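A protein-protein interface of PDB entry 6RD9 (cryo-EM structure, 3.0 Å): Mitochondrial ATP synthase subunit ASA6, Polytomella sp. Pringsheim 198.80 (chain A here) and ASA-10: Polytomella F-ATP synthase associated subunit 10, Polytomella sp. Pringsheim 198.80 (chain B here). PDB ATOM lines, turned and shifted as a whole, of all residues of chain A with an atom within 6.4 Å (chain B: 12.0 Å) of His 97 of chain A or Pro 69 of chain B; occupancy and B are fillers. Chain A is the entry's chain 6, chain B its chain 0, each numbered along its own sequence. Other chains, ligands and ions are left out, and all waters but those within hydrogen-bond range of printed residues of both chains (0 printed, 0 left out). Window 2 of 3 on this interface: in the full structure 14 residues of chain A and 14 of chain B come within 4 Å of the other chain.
Hydrophobic or aromatic side chains of chain B within 4 Å of the printed part of chain A: Pro 62, Phe 65, Pro 66 and Pro 69.
Of the 9 printed residues of chain A, 4 touch a printed residue of chain B.
Printed residues of chain A that touch a printed residue of chain B: Ser 94, Lys 95, His 97 and Trp 99.
Hydrophobic or aromatic side chains of chain A within 4 Å of the printed part of chain B: His 97 and Trp 99.
Gln 93 of chain A touches none of the printed residues of chain B.
Printed residues of chain B within 4 Å of Lys 95 of chain A: Pro 62, Thr 63 and Ala 64.
No residue of chain B comes within 4 Å of Ala 96 of chain A.
Of chain B, only Pro 69 comes within 4 Å of His 97 of chain A.
No residue of chain B comes within 4 Å of Glu 98 of chain A.
Printed residues of chain B within 4 Å of Trp 99 of chain A: Phe 65 (3.8 Å) and Pro 66 (3.3 Å).
Gln 60 of chain B touches none of the printed residues of chain A.
Of the printed residues of chain A, Pro 62 of chain B touches Lys 95 (3.8 Å).
Printed residues of chain A within 4 Å of Ala 64 of chain B: Ser 94 (2.8 Å) and Lys 95 (3.9 Å).
Of chain A, only His 97 comes within 4 Å of Pro 69 of chain B.
The nearest residue of chain A that does not touch Pro 69 of chain B is Trp 99 of chain A (5.4 Å).
The side-chain hydroxyl (OG) of Ser 94 of chain A sits at hydrogen-bond distance from the backbone carbonyl oxygen (O) of Ala 64 of chain B (3.0 Å).
The backbone carbonyl oxygen (O) of Pro 66 of chain B sits close to the indole nitrogen (NE1) of Trp 99 of chain A.
The backbone carbonyl oxygen (O) of Met 71 of chain B sits at hydrogen-bond distance from the backbone NH (N) of Thr 63 of chain B, at 2.9 Å.
The side-chain hydroxyl (OG1) of Thr 63 of chain B sits at hydrogen-bond distance from the side-chain carboxylate (OD1) of Asp 73 of chain B.
The backbone NH (N) of Lys 72 of chain B lies close to the side-chain hydroxyl (OG1) of Thr 63 of chain B, at 3.4 Å.
Among the printed residues, pairs that only touch across the chains: Ser 94 of chain A with Thr 63 of chain B (3.97 Å), Ser 94 of chain A with Phe 65 of chain B (3.7 Å), Ser 94 of chain A with Pro 66 of chain B (3.6 Å), Lys 95 of chain A with Pro 62 of chain B (3.8 Å), Lys 95 of chain A with Thr 63 of chain B (3.4 Å), Lys 95 of chain A with Ala 64 of chain B (3.9 Å), His 97 of chain A with Pro 69 of chain B (3.7 Å) and Trp 99 of chain A with Phe 65 of chain B (3.8 Å).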
ATOM      1  N   GLN A  93       3.296  -6.090  -1.901  1.00  0.00           N
ATOM      2  CA  GLN A  93       3.555  -5.420  -3.164  1.00  0.00           C
ATOM      3  C   GLN A  93       4.403  -6.263  -4.076  1.00  0.00           C
ATOM      4  O   GLN A  93       4.333  -6.101  -5.293  1.00  0.00           O
ATOM      5  CB  GLN A  93       4.286  -4.106  -2.954  1.00  0.00           C
ATOM      6  CG  GLN A  93       3.440  -2.891  -2.860  1.00  0.00           C
ATOM      7  CD  GLN A  93       4.280  -1.666  -2.786  1.00  0.00           C
ATOM      8  OE1 GLN A  93       5.488  -1.748  -2.636  1.00  0.00           O
ATOM      9  NE2 GLN A  93       3.654  -0.515  -2.892  1.00  0.00           N
ATOM     10  N   SER A  94       5.222  -7.134  -3.516  1.00  0.00           N
ATOM     11  CA  SER A  94       6.138  -7.934  -4.301  1.00  0.00           C
ATOM     12  C   SER A  94       5.502  -9.188  -4.851  1.00  0.00           C
ATOM     13  O   SER A  94       6.168  -9.920  -5.572  1.00  0.00           O
ATOM     14  CB  SER A  94       7.328  -8.313  -3.453  1.00  0.00           C
ATOM     15  OG  SER A  94       6.907  -9.155  -2.405  1.00  0.00           O
ATOM     16  N   LYS A  95       4.242  -9.447  -4.553  1.00  0.00           N
ATOM     17  CA  LYS A  95       3.531 -10.564  -5.138  1.00  0.00           C
ATOM     18  C   LYS A  95       2.191 -10.119  -5.688  1.00  0.00           C
ATOM     19  O   LYS A  95       1.183 -10.808  -5.550  1.00  0.00           O
ATOM     20  CB  LYS A  95       3.357 -11.672  -4.116  1.00  0.00           C
ATOM     21  CG  LYS A  95       2.853 -11.207  -2.811  1.00  0.00           C
ATOM     22  CD  LYS A  95       2.816 -12.312  -1.799  1.00  0.00           C
ATOM     23  CE  LYS A  95       4.157 -12.510  -1.157  1.00  0.00           C
ATOM     24  NZ  LYS A  95       3.975 -13.252   0.098  1.00  0.00           N
ATOM     25  N   ALA A  96       2.156  -8.976  -6.362  1.00  0.00           N
ATOM     26  CA  ALA A  96       0.900  -8.304  -6.645  1.00  0.00           C
ATOM     27  C   ALA A  96       0.464  -8.412  -8.092  1.00  0.00           C
ATOM     28  O   ALA A  96      -0.472  -7.709  -8.482  1.00  0.00           O
ATOM     29  CB  ALA A  96       1.003  -6.833  -6.263  1.00  0.00           C
ATOM     30  N   HIS A  97       1.156  -9.225  -8.895  1.00  0.00           N
ATOM     31  CA  HIS A  97       1.012  -9.464 -10.334  1.00  0.00           C
ATOM     32  C   HIS A  97       1.493  -8.294 -11.180  1.00  0.00           C
ATOM     33  O   HIS A  97       1.791  -8.460 -12.359  1.00  0.00           O
ATOM     34  CB  HIS A  97      -0.427  -9.833 -10.729  1.00  0.00           C
ATOM     35  CG  HIS A  97      -0.567 -10.251 -12.157  1.00  0.00           C
ATOM     36  ND1 HIS A  97      -0.209 -11.502 -12.602  1.00  0.00           N
ATOM     37  CD2 HIS A  97      -0.955  -9.557 -13.250  1.00  0.00           C
ATOM     38  CE1 HIS A  97      -0.404 -11.573 -13.904  1.00  0.00           C
ATOM     39  NE2 HIS A  97      -0.853 -10.404 -14.322  1.00  0.00           N
ATOM     40  N   GLU A  98       1.679  -7.137 -10.583  1.00  0.00           N
ATOM     41  CA  GLU A  98       2.325  -6.006 -11.216  1.00  0.00           C
ATOM     42  C   GLU A  98       3.442  -5.551 -10.325  1.00  0.00           C
ATOM     43  O   GLU A  98       3.646  -4.363 -10.095  1.00  0.00           O
ATOM     44  CB  GLU A  98       1.338  -4.881 -11.465  1.00  0.00           C
ATOM     45  CG  GLU A  98       0.183  -5.249 -12.362  1.00  0.00           C
ATOM     46  CD  GLU A  98       0.474  -4.999 -13.825  1.00  0.00           C
ATOM     47  OE1 GLU A  98       1.523  -4.400 -14.130  1.00  0.00           O
ATOM     48  OE2 GLU A  98      -0.345  -5.404 -14.674  1.00  0.00           O
ATOM     49  N   TRP A  99       4.176  -6.534  -9.809  1.00  0.00           N
ATOM     50  CA  TRP A  99       5.035  -6.344  -8.650  1.00  0.00           C
ATOM     51  C   TRP A  99       6.193  -5.421  -8.960  1.00  0.00           C
ATOM     52  O   TRP A  99       6.626  -4.659  -8.101  1.00  0.00           O
ATOM     53  CB  TRP A  99       5.554  -7.697  -8.167  1.00  0.00           C
ATOM     54  CG  TRP A  99       6.258  -8.446  -9.220  1.00  0.00           C
ATOM     55  CD1 TRP A  99       5.710  -9.272 -10.129  1.00  0.00           C
ATOM     56  CD2 TRP A  99       7.652  -8.416  -9.496  1.00  0.00           C
ATOM     57  NE1 TRP A  99       6.670  -9.764 -10.962  1.00  0.00           N
ATOM     58  CE2 TRP A  99       7.875  -9.244 -10.590  1.00  0.00           C
ATOM     59  CE3 TRP A  99       8.733  -7.755  -8.929  1.00  0.00           C
ATOM     60  CZ2 TRP A  99       9.123  -9.436 -11.119  1.00  0.00           C
ATOM     61  CZ3 TRP A  99       9.961  -7.945  -9.458  1.00  0.00           C
ATOM     62  CH2 TRP A  99      10.154  -8.778 -10.537  1.00  0.00           C
ATOM     63  N   ILE A 100       6.708  -5.467 -10.183  1.00  0.00           N
ATOM     64  CA  ILE A 100       7.810  -4.594 -10.534  1.00  0.00           C
ATOM     65  C   ILE A 100       7.293  -3.200 -10.824  1.00  0.00           C
ATOM     66  O   ILE A 100       8.021  -2.225 -10.650  1.00  0.00           O
ATOM     67  CB  ILE A 100       8.607  -5.219 -11.694  1.00  0.00           C
ATOM     68  CG1 ILE A 100       9.918  -4.488 -11.945  1.00  0.00           C
ATOM     69  CG2 ILE A 100       7.795  -5.280 -12.936  1.00  0.00           C
ATOM     70  CD1 ILE A 100      10.817  -4.454 -10.771  1.00  0.00           C
ATOM     71  N   ASP A 102       4.658  -1.998  -9.073  1.00  0.00           N
ATOM     72  CA  ASP A 102       4.356  -1.532  -7.725  1.00  0.00           C
ATOM     73  C   ASP A 102       5.614  -1.112  -6.994  1.00  0.00           C
ATOM     74  O   ASP A 102       5.620  -0.092  -6.310  1.00  0.00           O
ATOM     75  CB  ASP A 102       3.656  -2.614  -6.915  1.00  0.00           C
ATOM     76  CG  ASP A 102       2.267  -2.891  -7.392  1.00  0.00           C
ATOM     77  OD1 ASP A 102       1.939  -2.454  -8.498  1.00  0.00           O
ATOM     78  OD2 ASP A 102       1.500  -3.547  -6.665  1.00  0.00           O
ATOM     79  N   PRO B  58      -3.643 -22.785  -4.572  1.00  0.00           N
ATOM     80  CA  PRO B  58      -2.499 -22.129  -5.203  1.00  0.00           C
ATOM     81  C   PRO B  58      -2.692 -20.642  -5.378  1.00  0.00           C
ATOM     82  O   PRO B  58      -1.703 -19.908  -5.403  1.00  0.00           O
ATOM     83  CB  PRO B  58      -2.387 -22.843  -6.552  1.00  0.00           C
ATOM     84  CG  PRO B  58      -3.129 -24.085  -6.377  1.00  0.00           C
ATOM     85  CD  PRO B  58      -4.242 -23.782  -5.458  1.00  0.00           C
ATOM     86  N   ASP B  59      -3.934 -20.172  -5.489  1.00  0.00           N
ATOM     87  CA  ASP B  59      -4.176 -18.755  -5.718  1.00  0.00           C
ATOM     88  C   ASP B  59      -3.822 -17.917  -4.506  1.00  0.00           C
ATOM     89  O   ASP B  59      -3.470 -16.745  -4.650  1.00  0.00           O
ATOM     90  CB  ASP B  59      -5.634 -18.520  -6.089  1.00  0.00           C
ATOM     91  CG  ASP B  59      -5.875 -18.579  -7.572  1.00  0.00           C
ATOM     92  OD1 ASP B  59      -4.928 -18.310  -8.336  1.00  0.00           O
ATOM     93  OD2 ASP B  59      -7.014 -18.880  -7.979  1.00  0.00           O
ATOM     94  N   GLN B  60      -3.898 -18.492  -3.320  1.00  0.00           N
ATOM     95  CA  GLN B  60      -3.665 -17.760  -2.094  1.00  0.00           C
ATOM     96  C   GLN B  60      -2.209 -17.709  -1.688  1.00  0.00           C
ATOM     97  O   GLN B  60      -1.894 -17.093  -0.671  1.00  0.00           O
ATOM     98  CB  GLN B  60      -4.472 -18.373  -0.974  1.00  0.00           C
ATOM     99  CG  GLN B  60      -5.879 -18.606  -1.355  1.00  0.00           C
ATOM    100  CD  GLN B  60      -6.575 -17.339  -1.697  1.00  0.00           C
ATOM    101  OE1 GLN B  60      -7.231 -17.238  -2.718  1.00  0.00           O
ATOM    102  NE2 GLN B  60      -6.442 -16.350  -0.838  1.00  0.00           N
ATOM    103  N   HIS B  61      -1.313 -18.321  -2.443  1.00  0.00           N
ATOM    104  CA  HIS B  61       0.115 -18.262  -2.153  1.00  0.00           C
ATOM    105  C   HIS B  61       0.871 -17.870  -3.407  1.00  0.00           C
ATOM    106  O   HIS B  61       1.511 -18.717  -4.032  1.00  0.00           O
ATOM    107  CB  HIS B  61       0.632 -19.599  -1.635  1.00  0.00           C
ATOM    108  CG  HIS B  61      -0.076 -20.083  -0.417  1.00  0.00           C
ATOM    109  ND1 HIS B  61       0.482 -20.024   0.837  1.00  0.00           N
ATOM    110  CD2 HIS B  61      -1.300 -20.635  -0.261  1.00  0.00           C
ATOM    111  CE1 HIS B  61      -0.373 -20.512   1.716  1.00  0.00           C
ATOM    112  NE2 HIS B  61      -1.463 -20.886   1.075  1.00  0.00           N
ATOM    113  N   PRO B  62       0.835 -16.606  -3.801  1.00  0.00           N
ATOM    114  CA  PRO B  62       1.624 -16.186  -4.950  1.00  0.00           C
ATOM    115  C   PRO B  62       3.090 -16.056  -4.591  1.00  0.00           C
ATOM    116  O   PRO B  62       3.466 -15.901  -3.435  1.00  0.00           O
ATOM    117  CB  PRO B  62       1.024 -14.833  -5.309  1.00  0.00           C
ATOM    118  CG  PRO B  62       0.507 -14.339  -4.069  1.00  0.00           C
ATOM    119  CD  PRO B  62       0.050 -15.485  -3.270  1.00  0.00           C
ATOM    120  N   THR B  63       3.918 -16.155  -5.620  1.00  0.00           N
ATOM    121  CA  THR B  63       5.355 -16.200  -5.432  1.00  0.00           C
ATOM    122  C   THR B  63       5.875 -14.814  -5.096  1.00  0.00           C
ATOM    123  O   THR B  63       5.477 -13.823  -5.702  1.00  0.00           O
ATOM    124  CB  THR B  63       6.014 -16.766  -6.684  1.00  0.00           C
ATOM    125  OG1 THR B  63       5.667 -18.145  -6.784  1.00  0.00           O
ATOM    126  CG2 THR B  63       7.513 -16.670  -6.650  1.00  0.00           C
ATOM    127  N   ALA B  64       6.781 -14.763  -4.122  1.00  0.00           N
ATOM    128  CA  ALA B  64       7.186 -13.531  -3.476  1.00  0.00           C
ATOM    129  C   ALA B  64       7.906 -12.559  -4.384  1.00  0.00           C
ATOM    130  O   ALA B  64       8.023 -11.402  -4.010  1.00  0.00           O
ATOM    131  CB  ALA B  64       8.084 -13.852  -2.288  1.00  0.00           C
ATOM    132  N   PHE B  65       8.400 -12.973  -5.526  1.00  0.00           N
ATOM    133  CA  PHE B  65       9.052 -12.061  -6.459  1.00  0.00           C
ATOM    134  C   PHE B  65       9.061 -12.709  -7.828  1.00  0.00           C
ATOM    135  O   PHE B  65      10.145 -12.971  -8.361  1.00  0.00           O
ATOM    136  CB  PHE B  65      10.499 -11.783  -6.059  1.00  0.00           C
ATOM    137  CG  PHE B  65      10.702 -10.521  -5.302  1.00  0.00           C
ATOM    138  CD1 PHE B  65      10.644  -9.317  -5.944  1.00  0.00           C
ATOM    139  CD2 PHE B  65      11.007 -10.543  -3.959  1.00  0.00           C
ATOM    140  CE1 PHE B  65      10.851  -8.161  -5.258  1.00  0.00           C
ATOM    141  CE2 PHE B  65      11.198  -9.386  -3.272  1.00  0.00           C
ATOM    142  CZ  PHE B  65      11.122  -8.196  -3.923  1.00  0.00           C
ATOM    143  N   PRO B  66       7.902 -12.925  -8.445  1.00  0.00           N
ATOM    144  CA  PRO B  66       7.763 -14.031  -9.397  1.00  0.00           C
ATOM    145  C   PRO B  66       8.497 -13.784 -10.701  1.00  0.00           C
ATOM    146  O   PRO B  66       8.451 -12.691 -11.260  1.00  0.00           O
ATOM    147  CB  PRO B  66       6.253 -14.117  -9.612  1.00  0.00           C
ATOM    148  CG  PRO B  66       5.768 -12.786  -9.340  1.00  0.00           C
ATOM    149  CD  PRO B  66       6.659 -12.160  -8.322  1.00  0.00           C
ATOM    150  N   LYS B  67       9.213 -14.812 -11.153  1.00  0.00           N
ATOM    151  CA  LYS B  67       9.961 -14.710 -12.393  1.00  0.00           C
ATOM    152  C   LYS B  67       9.048 -14.774 -13.596  1.00  0.00           C
ATOM    153  O   LYS B  67       9.384 -14.246 -14.656  1.00  0.00           O
ATOM    154  CB  LYS B  67      10.999 -15.813 -12.461  1.00  0.00           C
ATOM    155  CG  LYS B  67      11.983 -15.802 -11.325  1.00  0.00           C
ATOM    156  CD  LYS B  67      12.805 -14.557 -11.378  1.00  0.00           C
ATOM    157  CE  LYS B  67      14.047 -14.674 -10.555  1.00  0.00           C
ATOM    158  NZ  LYS B  67      14.931 -13.519 -10.816  1.00  0.00           N
ATOM    159  N   VAL B  68       7.907 -15.437 -13.467  1.00  0.00           N
ATOM    160  CA  VAL B  68       6.864 -15.431 -14.480  1.00  0.00           C
ATOM    161  C   VAL B  68       5.578 -14.994 -13.795  1.00  0.00           C
ATOM    162  O   VAL B  68       5.260 -15.508 -12.723  1.00  0.00           O
ATOM    163  CB  VAL B  68       6.683 -16.806 -15.148  1.00  0.00           C
ATOM    164  CG1 VAL B  68       5.567 -16.775 -16.138  1.00  0.00           C
ATOM    165  CG2 VAL B  68       7.945 -17.199 -15.839  1.00  0.00           C
ATOM    166  N   PRO B  69       4.845 -14.033 -14.343  1.00  0.00           N
ATOM    167  CA  PRO B  69       3.604 -13.582 -13.713  1.00  0.00           C
ATOM    168  C   PRO B  69       2.539 -14.651 -13.605  1.00  0.00           C
ATOM    169  O   PRO B  69       1.970 -15.089 -14.603  1.00  0.00           O
ATOM    170  CB  PRO B  69       3.153 -12.455 -14.641  1.00  0.00           C
ATOM    171  CG  PRO B  69       4.376 -11.997 -15.276  1.00  0.00           C
ATOM    172  CD  PRO B  69       5.214 -13.174 -15.470  1.00  0.00           C
ATOM    173  N   GLY B  70       2.259 -15.060 -12.378  1.00  0.00           N
ATOM    174  CA  GLY B  70       1.321 -16.126 -12.112  1.00  0.00           C
ATOM    175  C   GLY B  70       1.922 -17.292 -11.380  1.00  0.00           C
ATOM    176  O   GLY B  70       1.220 -18.284 -11.154  1.00  0.00           O
ATOM    177  N   MET B  71       3.198 -17.223 -11.017  1.00  0.00           N
ATOM    178  CA  MET B  71       3.835 -18.289 -10.266  1.00  0.00           C
ATOM    179  C   MET B  71       3.277 -18.330  -8.861  1.00  0.00           C
ATOM    180  O   MET B  71       3.122 -17.295  -8.218  1.00  0.00           O
ATOM    181  CB  MET B  71       5.333 -18.068 -10.202  1.00  0.00           C
ATOM    182  CG  MET B  71       6.077 -18.480 -11.416  1.00  0.00           C
ATOM    183  SD  MET B  71       7.830 -18.271 -11.165  1.00  0.00           S
ATOM    184  CE  MET B  71       8.007 -19.029  -9.561  1.00  0.00           C
ATOM    185  N   LYS B  72       2.957 -19.523  -8.393  1.00  0.00           N
ATOM    186  CA  LYS B  72       2.434 -19.726  -7.059  1.00  0.00           C
ATOM    187  C   LYS B  72       3.398 -20.597  -6.279  1.00  0.00           C
ATOM    188  O   LYS B  72       4.198 -21.336  -6.850  1.00  0.00           O
ATOM    189  CB  LYS B  72       1.052 -20.363  -7.103  1.00  0.00           C
ATOM    190  CG  LYS B  72       0.127 -19.722  -8.102  1.00  0.00           C
ATOM    191  CD  LYS B  72      -0.123 -18.276  -7.768  1.00  0.00           C
ATOM    192  CE  LYS B  72      -1.144 -17.660  -8.687  1.00  0.00           C
ATOM    193  NZ  LYS B  72      -1.433 -16.256  -8.322  1.00  0.00           N
ATOM    194  N   ASP B  73       3.337 -20.494  -4.962  1.00  0.00           N
ATOM    195  CA  ASP B  73       4.301 -21.202  -4.141  1.00  0.00           C
ATOM    196  C   ASP B  73       3.866 -22.611  -3.800  1.00  0.00           C
ATOM    197  O   ASP B  73       4.705 -23.511  -3.738  1.00  0.00           O
ATOM    198  CB  ASP B  73       4.566 -20.432  -2.853  1.00  0.00           C
ATOM    199  CG  ASP B  73       5.599 -19.366  -3.033  1.00  0.00           C
ATOM    200  OD1 ASP B  73       6.124 -19.242  -4.157  1.00  0.00           O
ATOM    201  OD2 ASP B  73       5.895 -18.653  -2.057  1.00  0.00           O
